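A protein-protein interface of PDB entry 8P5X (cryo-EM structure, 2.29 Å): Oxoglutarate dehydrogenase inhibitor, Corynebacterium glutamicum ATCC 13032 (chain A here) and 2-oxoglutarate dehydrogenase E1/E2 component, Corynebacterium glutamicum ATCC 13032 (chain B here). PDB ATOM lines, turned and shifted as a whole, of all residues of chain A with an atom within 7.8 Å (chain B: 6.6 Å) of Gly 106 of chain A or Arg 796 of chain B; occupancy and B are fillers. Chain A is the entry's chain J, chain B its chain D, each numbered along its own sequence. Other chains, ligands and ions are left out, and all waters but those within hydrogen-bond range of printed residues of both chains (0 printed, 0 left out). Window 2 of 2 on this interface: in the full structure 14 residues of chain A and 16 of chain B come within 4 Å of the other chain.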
ATOM      1  N   SER A  87       7.874   9.917  17.462  1.00  0.00           N
ATOM      2  CA  SER A  87       6.911   8.811  17.240  1.00  0.00           C
ATOM      3  C   SER A  87       6.240   8.449  18.556  1.00  0.00           C
ATOM      4  O   SER A  87       6.831   8.739  19.610  1.00  0.00           O
ATOM      5  CB  SER A  87       7.601   7.625  16.665  1.00  0.00           C
ATOM      6  OG  SER A  87       8.244   7.958  15.444  1.00  0.00           O
ATOM      7  N   ARG A  88       5.071   7.815  18.493  1.00  0.00           N
ATOM      8  CA  ARG A  88       4.211   7.529  19.667  1.00  0.00           C
ATOM      9  C   ARG A  88       4.973   6.649  20.644  1.00  0.00           C
ATOM     10  O   ARG A  88       4.972   6.973  21.839  1.00  0.00           O
ATOM     11  CB  ARG A  88       2.902   6.853  19.258  1.00  0.00           C
ATOM     12  CG  ARG A  88       1.812   7.818  18.811  1.00  0.00           C
ATOM     13  CD  ARG A  88       0.410   7.263  19.016  1.00  0.00           C
ATOM     14  NE  ARG A  88      -0.491   8.309  19.481  1.00  0.00           N
ATOM     15  CZ  ARG A  88      -1.523   8.143  20.308  1.00  0.00           C
ATOM     16  NH1 ARG A  88      -1.832   6.951  20.799  1.00  0.00           N
ATOM     17  NH2 ARG A  88      -2.253   9.194  20.648  1.00  0.00           N
ATOM     18  N   ARG A  89       5.589   5.580  20.152  1.00  0.00           N
ATOM     19  CA  ARG A  89       6.601   4.782  20.884  1.00  0.00           C
ATOM     20  C   ARG A  89       7.929   4.950  20.151  1.00  0.00           C
ATOM     21  O   ARG A  89       7.968   4.543  18.990  1.00  0.00           O
ATOM     22  CB  ARG A  89       6.159   3.322  20.951  1.00  0.00           C
ATOM     23  CG  ARG A  89       4.804   3.095  21.606  1.00  0.00           C
ATOM     24  CD  ARG A  89       4.757   3.491  23.066  1.00  0.00           C
ATOM     25  NE  ARG A  89       3.498   3.119  23.701  1.00  0.00           N
ATOM     26  CZ  ARG A  89       3.128   3.456  24.937  1.00  0.00           C
ATOM     27  NH1 ARG A  89       3.915   4.189  25.712  1.00  0.00           N
ATOM     28  NH2 ARG A  89       1.952   3.058  25.399  1.00  0.00           N
ATOM     29  N   HIS A  90       8.960   5.542  20.783  1.00  0.00           N
ATOM     30  CA  HIS A  90      10.206   6.018  20.114  1.00  0.00           C
ATOM     31  C   HIS A  90      11.460   5.384  20.691  1.00  0.00           C
ATOM     32  O   HIS A  90      12.280   4.917  19.882  1.00  0.00           O
ATOM     33  CB  HIS A  90      10.334   7.529  20.167  1.00  0.00           C
ATOM     34  CG  HIS A  90      11.298   8.093  19.183  1.00  0.00           C
ATOM     35  ND1 HIS A  90      10.921   8.962  18.218  1.00  0.00           N
ATOM     36  CD2 HIS A  90      12.625   7.957  19.043  1.00  0.00           C
ATOM     37  CE1 HIS A  90      11.963   9.321  17.512  1.00  0.00           C
ATOM     38  NE2 HIS A  90      13.015   8.720  17.989  1.00  0.00           N
ATOM     39  N   ALA A  91      11.651   5.382  22.004  1.00  0.00           N
ATOM     40  CA  ALA A  91      12.799   4.697  22.627  1.00  0.00           C
ATOM     41  C   ALA A  91      12.523   4.347  24.076  1.00  0.00           C
ATOM     42  O   ALA A  91      11.633   4.963  24.664  1.00  0.00           O
ATOM     43  CB  ALA A  91      13.992   5.576  22.513  1.00  0.00           C
ATOM     44  N   VAL A 103      17.727   2.320  23.703  1.00  0.00           N
ATOM     45  CA  VAL A 103      17.246   1.324  22.700  1.00  0.00           C
ATOM     46  C   VAL A 103      16.165   1.960  21.845  1.00  0.00           C
ATOM     47  O   VAL A 103      15.200   2.454  22.428  1.00  0.00           O
ATOM     48  CB  VAL A 103      16.689   0.087  23.395  1.00  0.00           C
ATOM     49  CG1 VAL A 103      16.332  -0.981  22.386  1.00  0.00           C
ATOM     50  CG2 VAL A 103      17.651  -0.450  24.431  1.00  0.00           C
ATOM     51  N   ASP A 104      16.308   1.938  20.524  1.00  0.00           N
ATOM     52  CA  ASP A 104      15.257   2.382  19.576  1.00  0.00           C
ATOM     53  C   ASP A 104      14.235   1.260  19.436  1.00  0.00           C
ATOM     54  O   ASP A 104      14.659   0.121  19.179  1.00  0.00           O
ATOM     55  CB  ASP A 104      15.831   2.727  18.207  1.00  0.00           C
ATOM     56  CG  ASP A 104      14.871   3.519  17.344  1.00  0.00           C
ATOM     57  OD1 ASP A 104      14.704   4.732  17.613  1.00  0.00           O
ATOM     58  OD2 ASP A 104      14.287   2.920  16.415  1.00  0.00           O
ATOM     59  N   VAL A 105      12.948   1.578  19.591  1.00  0.00           N
ATOM     60  CA  VAL A 105      11.822   0.605  19.565  1.00  0.00           C
ATOM     61  C   VAL A 105      11.001   0.776  18.281  1.00  0.00           C
ATOM     62  O   VAL A 105       9.809   0.433  18.300  1.00  0.00           O
ATOM     63  CB  VAL A 105      10.965   0.747  20.829  1.00  0.00           C
ATOM     64  CG1 VAL A 105      11.826   0.652  22.075  1.00  0.00           C
ATOM     65  CG2 VAL A 105      10.144   2.029  20.844  1.00  0.00           C
ATOM     66  N   GLY A 106      11.610   1.265  17.198  1.00  0.00           N
ATOM     67  CA  GLY A 106      11.056   1.207  15.836  1.00  0.00           C
ATOM     68  C   GLY A 106      10.463   2.523  15.387  1.00  0.00           C
ATOM     69  O   GLY A 106       9.329   2.512  14.886  1.00  0.00           O
ATOM     70  N   SER A 107      11.212   3.610  15.517  1.00  0.00           N
ATOM     71  CA  SER A 107      10.789   4.980  15.152  1.00  0.00           C
ATOM     72  C   SER A 107      11.163   5.265  13.708  1.00  0.00           C
ATOM     73  O   SER A 107      12.030   4.560  13.183  1.00  0.00           O
ATOM     74  CB  SER A 107      11.408   5.980  16.065  1.00  0.00           C
ATOM     75  OG  SER A 107      12.830   5.904  16.008  1.00  0.00           O
ATOM     76  N   LEU A 108      10.555   6.279  13.107  1.00  0.00           N
ATOM     77  CA  LEU A 108      10.784   6.652  11.699  1.00  0.00           C
ATOM     78  C   LEU A 108      12.114   7.378  11.569  1.00  0.00           C
ATOM     79  O   LEU A 108      12.883   7.024  10.649  1.00  0.00           O
ATOM     80  CB  LEU A 108       9.642   7.537  11.217  1.00  0.00           C
ATOM     81  CG  LEU A 108       9.692   7.941   9.751  1.00  0.00           C
ATOM     82  CD1 LEU A 108       9.521   6.737   8.856  1.00  0.00           C
ATOM     83  CD2 LEU A 108       8.631   8.975   9.446  1.00  0.00           C
ATOM     84  N   ASN A 109      12.374   8.355  12.437  1.00  0.00           N
ATOM     85  CA  ASN A 109      13.558   9.243  12.354  1.00  0.00           C
ATOM     86  C   ASN A 109      14.768   8.613  13.046  1.00  0.00           C
ATOM     87  O   ASN A 109      15.888   9.063  12.764  1.00  0.00           O
ATOM     88  CB  ASN A 109      13.261  10.623  12.931  1.00  0.00           C
ATOM     89  CG  ASN A 109      12.449  11.507  12.012  1.00  0.00           C
ATOM     90  OD1 ASN A 109      12.589  11.454  10.797  1.00  0.00           O
ATOM     91  ND2 ASN A 109      11.615  12.355  12.587  1.00  0.00           N
ATOM     92  N   GLY A 110      14.572   7.641  13.928  1.00  0.00           N
ATOM     93  CA  GLY A 110      15.666   6.949  14.623  1.00  0.00           C
ATOM     94  C   GLY A 110      16.183   7.739  15.800  1.00  0.00           C
ATOM     95  O   GLY A 110      15.743   8.879  15.975  1.00  0.00           O
ATOM     96  N   THR A 111      17.092   7.144  16.575  1.00  0.00           N
ATOM     97  CA  THR A 111      17.793   7.743  17.739  1.00  0.00           C
ATOM     98  C   THR A 111      19.276   7.919  17.423  1.00  0.00           C
ATOM     99  O   THR A 111      19.870   6.967  16.905  1.00  0.00           O
ATOM    100  CB  THR A 111      17.653   6.843  18.957  1.00  0.00           C
ATOM    101  OG1 THR A 111      16.266   6.561  19.122  1.00  0.00           O
ATOM    102  CG2 THR A 111      18.191   7.474  20.216  1.00  0.00           C
ATOM    103  N   ASN A 119      21.130   1.740  17.247  1.00  0.00           N
ATOM    104  CA  ASN A 119      19.945   0.909  17.575  1.00  0.00           C
ATOM    105  C   ASN A 119      19.946   0.568  19.060  1.00  0.00           C
ATOM    106  O   ASN A 119      18.850   0.500  19.640  1.00  0.00           O
ATOM    107  CB  ASN A 119      19.907  -0.370  16.754  1.00  0.00           C
ATOM    108  CG  ASN A 119      19.686  -0.101  15.283  1.00  0.00           C
ATOM    109  OD1 ASN A 119      19.890   1.018  14.813  1.00  0.00           O
ATOM    110  ND2 ASN A 119      19.273  -1.123  14.550  1.00  0.00           N
ATOM    111  N   ASN B 493       2.593  13.742   5.706  1.00  0.00           N
ATOM    112  CA  ASN B 493       1.636  13.014   6.565  1.00  0.00           C
ATOM    113  C   ASN B 493       0.929  13.988   7.482  1.00  0.00           C
ATOM    114  O   ASN B 493      -0.285  13.846   7.643  1.00  0.00           O
ATOM    115  CB  ASN B 493       2.296  11.945   7.417  1.00  0.00           C
ATOM    116  CG  ASN B 493       2.647  10.694   6.657  1.00  0.00           C
ATOM    117  OD1 ASN B 493       2.366  10.571   5.471  1.00  0.00           O
ATOM    118  ND2 ASN B 493       3.275   9.753   7.331  1.00  0.00           N
ATOM    119  N   GLU B 789      12.032  -3.797   8.575  1.00  0.00           N
ATOM    120  CA  GLU B 789      11.752  -2.977   9.785  1.00  0.00           C
ATOM    121  C   GLU B 789      11.459  -1.528   9.378  1.00  0.00           C
ATOM    122  O   GLU B 789      10.539  -0.928   9.965  1.00  0.00           O
ATOM    123  CB  GLU B 789      12.931  -3.035  10.758  1.00  0.00           C
ATOM    124  CG  GLU B 789      13.140  -4.409  11.375  1.00  0.00           C
ATOM    125  CD  GLU B 789      14.192  -4.474  12.473  1.00  0.00           C
ATOM    126  OE1 GLU B 789      15.171  -3.697  12.410  1.00  0.00           O
ATOM    127  OE2 GLU B 789      14.030  -5.305  13.395  1.00  0.00           O
ATOM    128  N   ALA B 791      10.318  -0.421   6.430  1.00  0.00           N
ATOM    129  CA  ALA B 791       9.096  -0.384   5.610  1.00  0.00           C
ATOM    130  C   ALA B 791       7.853  -0.341   6.488  1.00  0.00           C
ATOM    131  O   ALA B 791       6.915   0.379   6.115  1.00  0.00           O
ATOM    132  CB  ALA B 791       9.067  -1.576   4.702  1.00  0.00           C
ATOM    133  N   GLU B 792       7.826  -1.099   7.585  1.00  0.00           N
ATOM    134  CA  GLU B 792       6.699  -1.126   8.555  1.00  0.00           C
ATOM    135  C   GLU B 792       6.490   0.255   9.175  1.00  0.00           C
ATOM    136  O   GLU B 792       5.333   0.611   9.440  1.00  0.00           O
ATOM    137  CB  GLU B 792       6.974  -2.110   9.688  1.00  0.00           C
ATOM    138  CG  GLU B 792       6.902  -3.560   9.267  1.00  0.00           C
ATOM    139  CD  GLU B 792       7.386  -4.543  10.323  1.00  0.00           C
ATOM    140  OE1 GLU B 792       7.221  -4.247  11.532  1.00  0.00           O
ATOM    141  OE2 GLU B 792       7.927  -5.609   9.938  1.00  0.00           O
ATOM    142  N   ALA B 793       7.575   0.982   9.422  1.00  0.00           N
ATOM    143  CA  ALA B 793       7.591   2.296  10.092  1.00  0.00           C
ATOM    144  C   ALA B 793       6.903   3.341   9.229  1.00  0.00           C
ATOM    145  O   ALA B 793       6.203   4.190   9.801  1.00  0.00           O
ATOM    146  CB  ALA B 793       9.006   2.712  10.380  1.00  0.00           C
ATOM    147  N   VAL B 794       7.117   3.301   7.919  1.00  0.00           N
ATOM    148  CA  VAL B 794       6.530   4.276   6.956  1.00  0.00           C
ATOM    149  C   VAL B 794       5.004   4.204   7.034  1.00  0.00           C
ATOM    150  O   VAL B 794       4.359   5.264   6.977  1.00  0.00           O
ATOM    151  CB  VAL B 794       7.056   4.030   5.533  1.00  0.00           C
ATOM    152  CG1 VAL B 794       6.224   4.744   4.472  1.00  0.00           C
ATOM    153  CG2 VAL B 794       8.521   4.416   5.413  1.00  0.00           C
ATOM    154  N   VAL B 795       4.452   3.009   7.209  1.00  0.00           N
ATOM    155  CA  VAL B 795       2.985   2.759   7.265  1.00  0.00           C
ATOM    156  C   VAL B 795       2.415   3.310   8.565  1.00  0.00           C
ATOM    157  O   VAL B 795       1.339   3.912   8.533  1.00  0.00           O
ATOM    158  CB  VAL B 795       2.697   1.258   7.136  1.00  0.00           C
ATOM    159  CG1 VAL B 795       1.202   0.963   7.228  1.00  0.00           C
ATOM    160  CG2 VAL B 795       3.293   0.688   5.854  1.00  0.00           C
ATOM    161  N   ARG B 796       3.120   3.107   9.664  1.00  0.00           N
ATOM    162  CA  ARG B 796       2.671   3.386  11.044  1.00  0.00           C
ATOM    163  C   ARG B 796       2.709   4.876  11.338  1.00  0.00           C
ATOM    164  O   ARG B 796       2.030   5.285  12.290  1.00  0.00           O
ATOM    165  CB  ARG B 796       3.619   2.658  11.989  1.00  0.00           C
ATOM    166  CG  ARG B 796       3.091   2.375  13.383  1.00  0.00           C
ATOM    167  CD  ARG B 796       3.774   1.135  13.930  1.00  0.00           C
ATOM    168  NE  ARG B 796       5.217   1.214  13.776  1.00  0.00           N
ATOM    169  CZ  ARG B 796       6.052   0.186  13.694  1.00  0.00           C
ATOM    170  NH1 ARG B 796       5.612  -1.058  13.740  1.00  0.00           N
ATOM    171  NH2 ARG B 796       7.345   0.405  13.548  1.00  0.00           N
ATOM    172  N   ASP B 797       3.493   5.654  10.585  1.00  0.00           N
ATOM    173  CA  ASP B 797       3.684   7.107  10.820  1.00  0.00           C
ATOM    174  C   ASP B 797       2.378   7.852  10.572  1.00  0.00           C
ATOM    175  O   ASP B 797       2.084   8.765  11.360  1.00  0.00           O
ATOM    176  CB  ASP B 797       4.777   7.710   9.939  1.00  0.00           C
ATOM    177  CG  ASP B 797       5.142   9.139  10.323  1.00  0.00           C
ATOM    178  OD1 ASP B 797       5.598   9.345  11.472  1.00  0.00           O
ATOM    179  OD2 ASP B 797       4.963  10.043   9.472  1.00  0.00           O
ATOM    180  N   PHE B 798       1.631   7.496   9.527  1.00  0.00           N
ATOM    181  CA  PHE B 798       0.368   8.180   9.159  1.00  0.00           C
ATOM    182  C   PHE B 798      -0.697   7.920  10.215  1.00  0.00           C
ATOM    183  O   PHE B 798      -1.492   8.830  10.461  1.00  0.00           O
ATOM    184  CB  PHE B 798      -0.119   7.769   7.774  1.00  0.00           C
ATOM    185  CG  PHE B 798      -1.227   8.637   7.235  1.00  0.00           C
ATOM    186  CD1 PHE B 798      -1.067  10.007   7.131  1.00  0.00           C
ATOM    187  CD2 PHE B 798      -2.433   8.095   6.843  1.00  0.00           C
ATOM    188  CE1 PHE B 798      -2.091  10.812   6.662  1.00  0.00           C
ATOM    189  CE2 PHE B 798      -3.451   8.900   6.369  1.00  0.00           C
ATOM    190  CZ  PHE B 798      -3.279  10.256   6.279  1.00  0.00           C
ATOM    191  N   HIS B 799      -0.711   6.751  10.837  1.00  0.00           N
ATOM    192  CA  HIS B 799      -1.668   6.418  11.916  1.00  0.00           C
ATOM    193  C   HIS B 799      -1.318   7.193  13.178  1.00  0.00           C
ATOM    194  O   HIS B 799      -2.256   7.593  13.885  1.00  0.00           O
ATOM    195  CB  HIS B 799      -1.719   4.912  12.160  1.00  0.00           C
ATOM    196  CG  HIS B 799      -2.321   4.168  11.016  1.00  0.00           C
ATOM    197  ND1 HIS B 799      -3.682   4.185  10.763  1.00  0.00           N
ATOM    198  CD2 HIS B 799      -1.760   3.416  10.041  1.00  0.00           C
ATOM    199  CE1 HIS B 799      -3.936   3.462   9.688  1.00  0.00           C
ATOM    200  NE2 HIS B 799      -2.772   2.977   9.226  1.00  0.00           N
ATOM    201  N   ASP B 800      -0.031   7.387  13.460  1.00  0.00           N
ATOM    202  CA  ASP B 800       0.446   8.144  14.644  1.00  0.00           C
ATOM    203  C   ASP B 800      -0.023   9.593  14.549  1.00  0.00           C
ATOM    204  O   ASP B 800      -0.604  10.075  15.529  1.00  0.00           O
ATOM    205  CB  ASP B 800       1.969   8.104  14.777  1.00  0.00           C
ATOM    206  CG  ASP B 800       2.537   6.790  15.290  1.00  0.00           C
ATOM    207  OD1 ASP B 800       1.788   6.033  15.951  1.00  0.00           O
ATOM    208  OD2 ASP B 800       3.737   6.539  15.035  1.00  0.00           O
ATOM    209  N   GLN B 801       0.226  10.260  13.423  1.00  0.00           N
ATOM    210  CA  GLN B 801      -0.090  11.696  13.237  1.00  0.00           C
ATOM    211  C   GLN B 801      -1.590  11.904  13.416  1.00  0.00           C
ATOM    212  O   GLN B 801      -1.968  12.930  14.017  1.00  0.00           O
ATOM    213  CB  GLN B 801       0.300  12.214  11.859  1.00  0.00           C
ATOM    214  CG  GLN B 801       1.778  12.089  11.522  1.00  0.00           C
ATOM    215  CD  GLN B 801       2.666  13.080  12.218  1.00  0.00           C
ATOM    216  OE1 GLN B 801       2.221  14.095  12.747  1.00  0.00           O
ATOM    217  NE2 GLN B 801       3.955  12.792  12.203  1.00  0.00           N
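Printed residues of chain B within 4 Å of Arg 88 of chain A: Asp 800. Of the printed residues of chain B, Leu 108 of chain A touches Asp 797 (3.6 Å). Arg 796 of chain B touches one residue of chain A. Of the printed residues of chain A, Asp 797 of chain B touches Leu 108 (3.6 Å). Of the printed residues of chain A, Asp 800 of chain B touches Arg 88 (3.4 Å). The nearest residue of chain A that does not touch Arg 796 of chain B is Val 105 of chain A (5.4 Å).
Hydrophobic or aromatic side chains of chain A that line the printed part of chain B: Leu 108. Among the printed residues, 3 pairs touch across the chains. Among the printed residues, no Asp or Glu carboxylate lies within 4 Å of a Lys or Arg side-chain nitrogen of the other chain.
O of Gly 106 of chain A sits at hydrogen-bond distance from NH2 of Arg 796 of chain B (3.2 Å).
Among the printed residues, pairs that only touch across the chains: Arg 88 of chain A with Asp 800 of chain B (3.4 Å) and Leu 108 of chain A with Asp 797 of chain B (3.6 Å).
ND2 of Asn 493 of chain B sits at hydrogen-bond distance from OD2 of Asp 797 of chain B, at 2.7 Å. The backbone NH of Gly 106 of chain A lies within hydrogen-bond range of the side-chain carboxylate of Asp 104 of chain A (3.2 Å).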
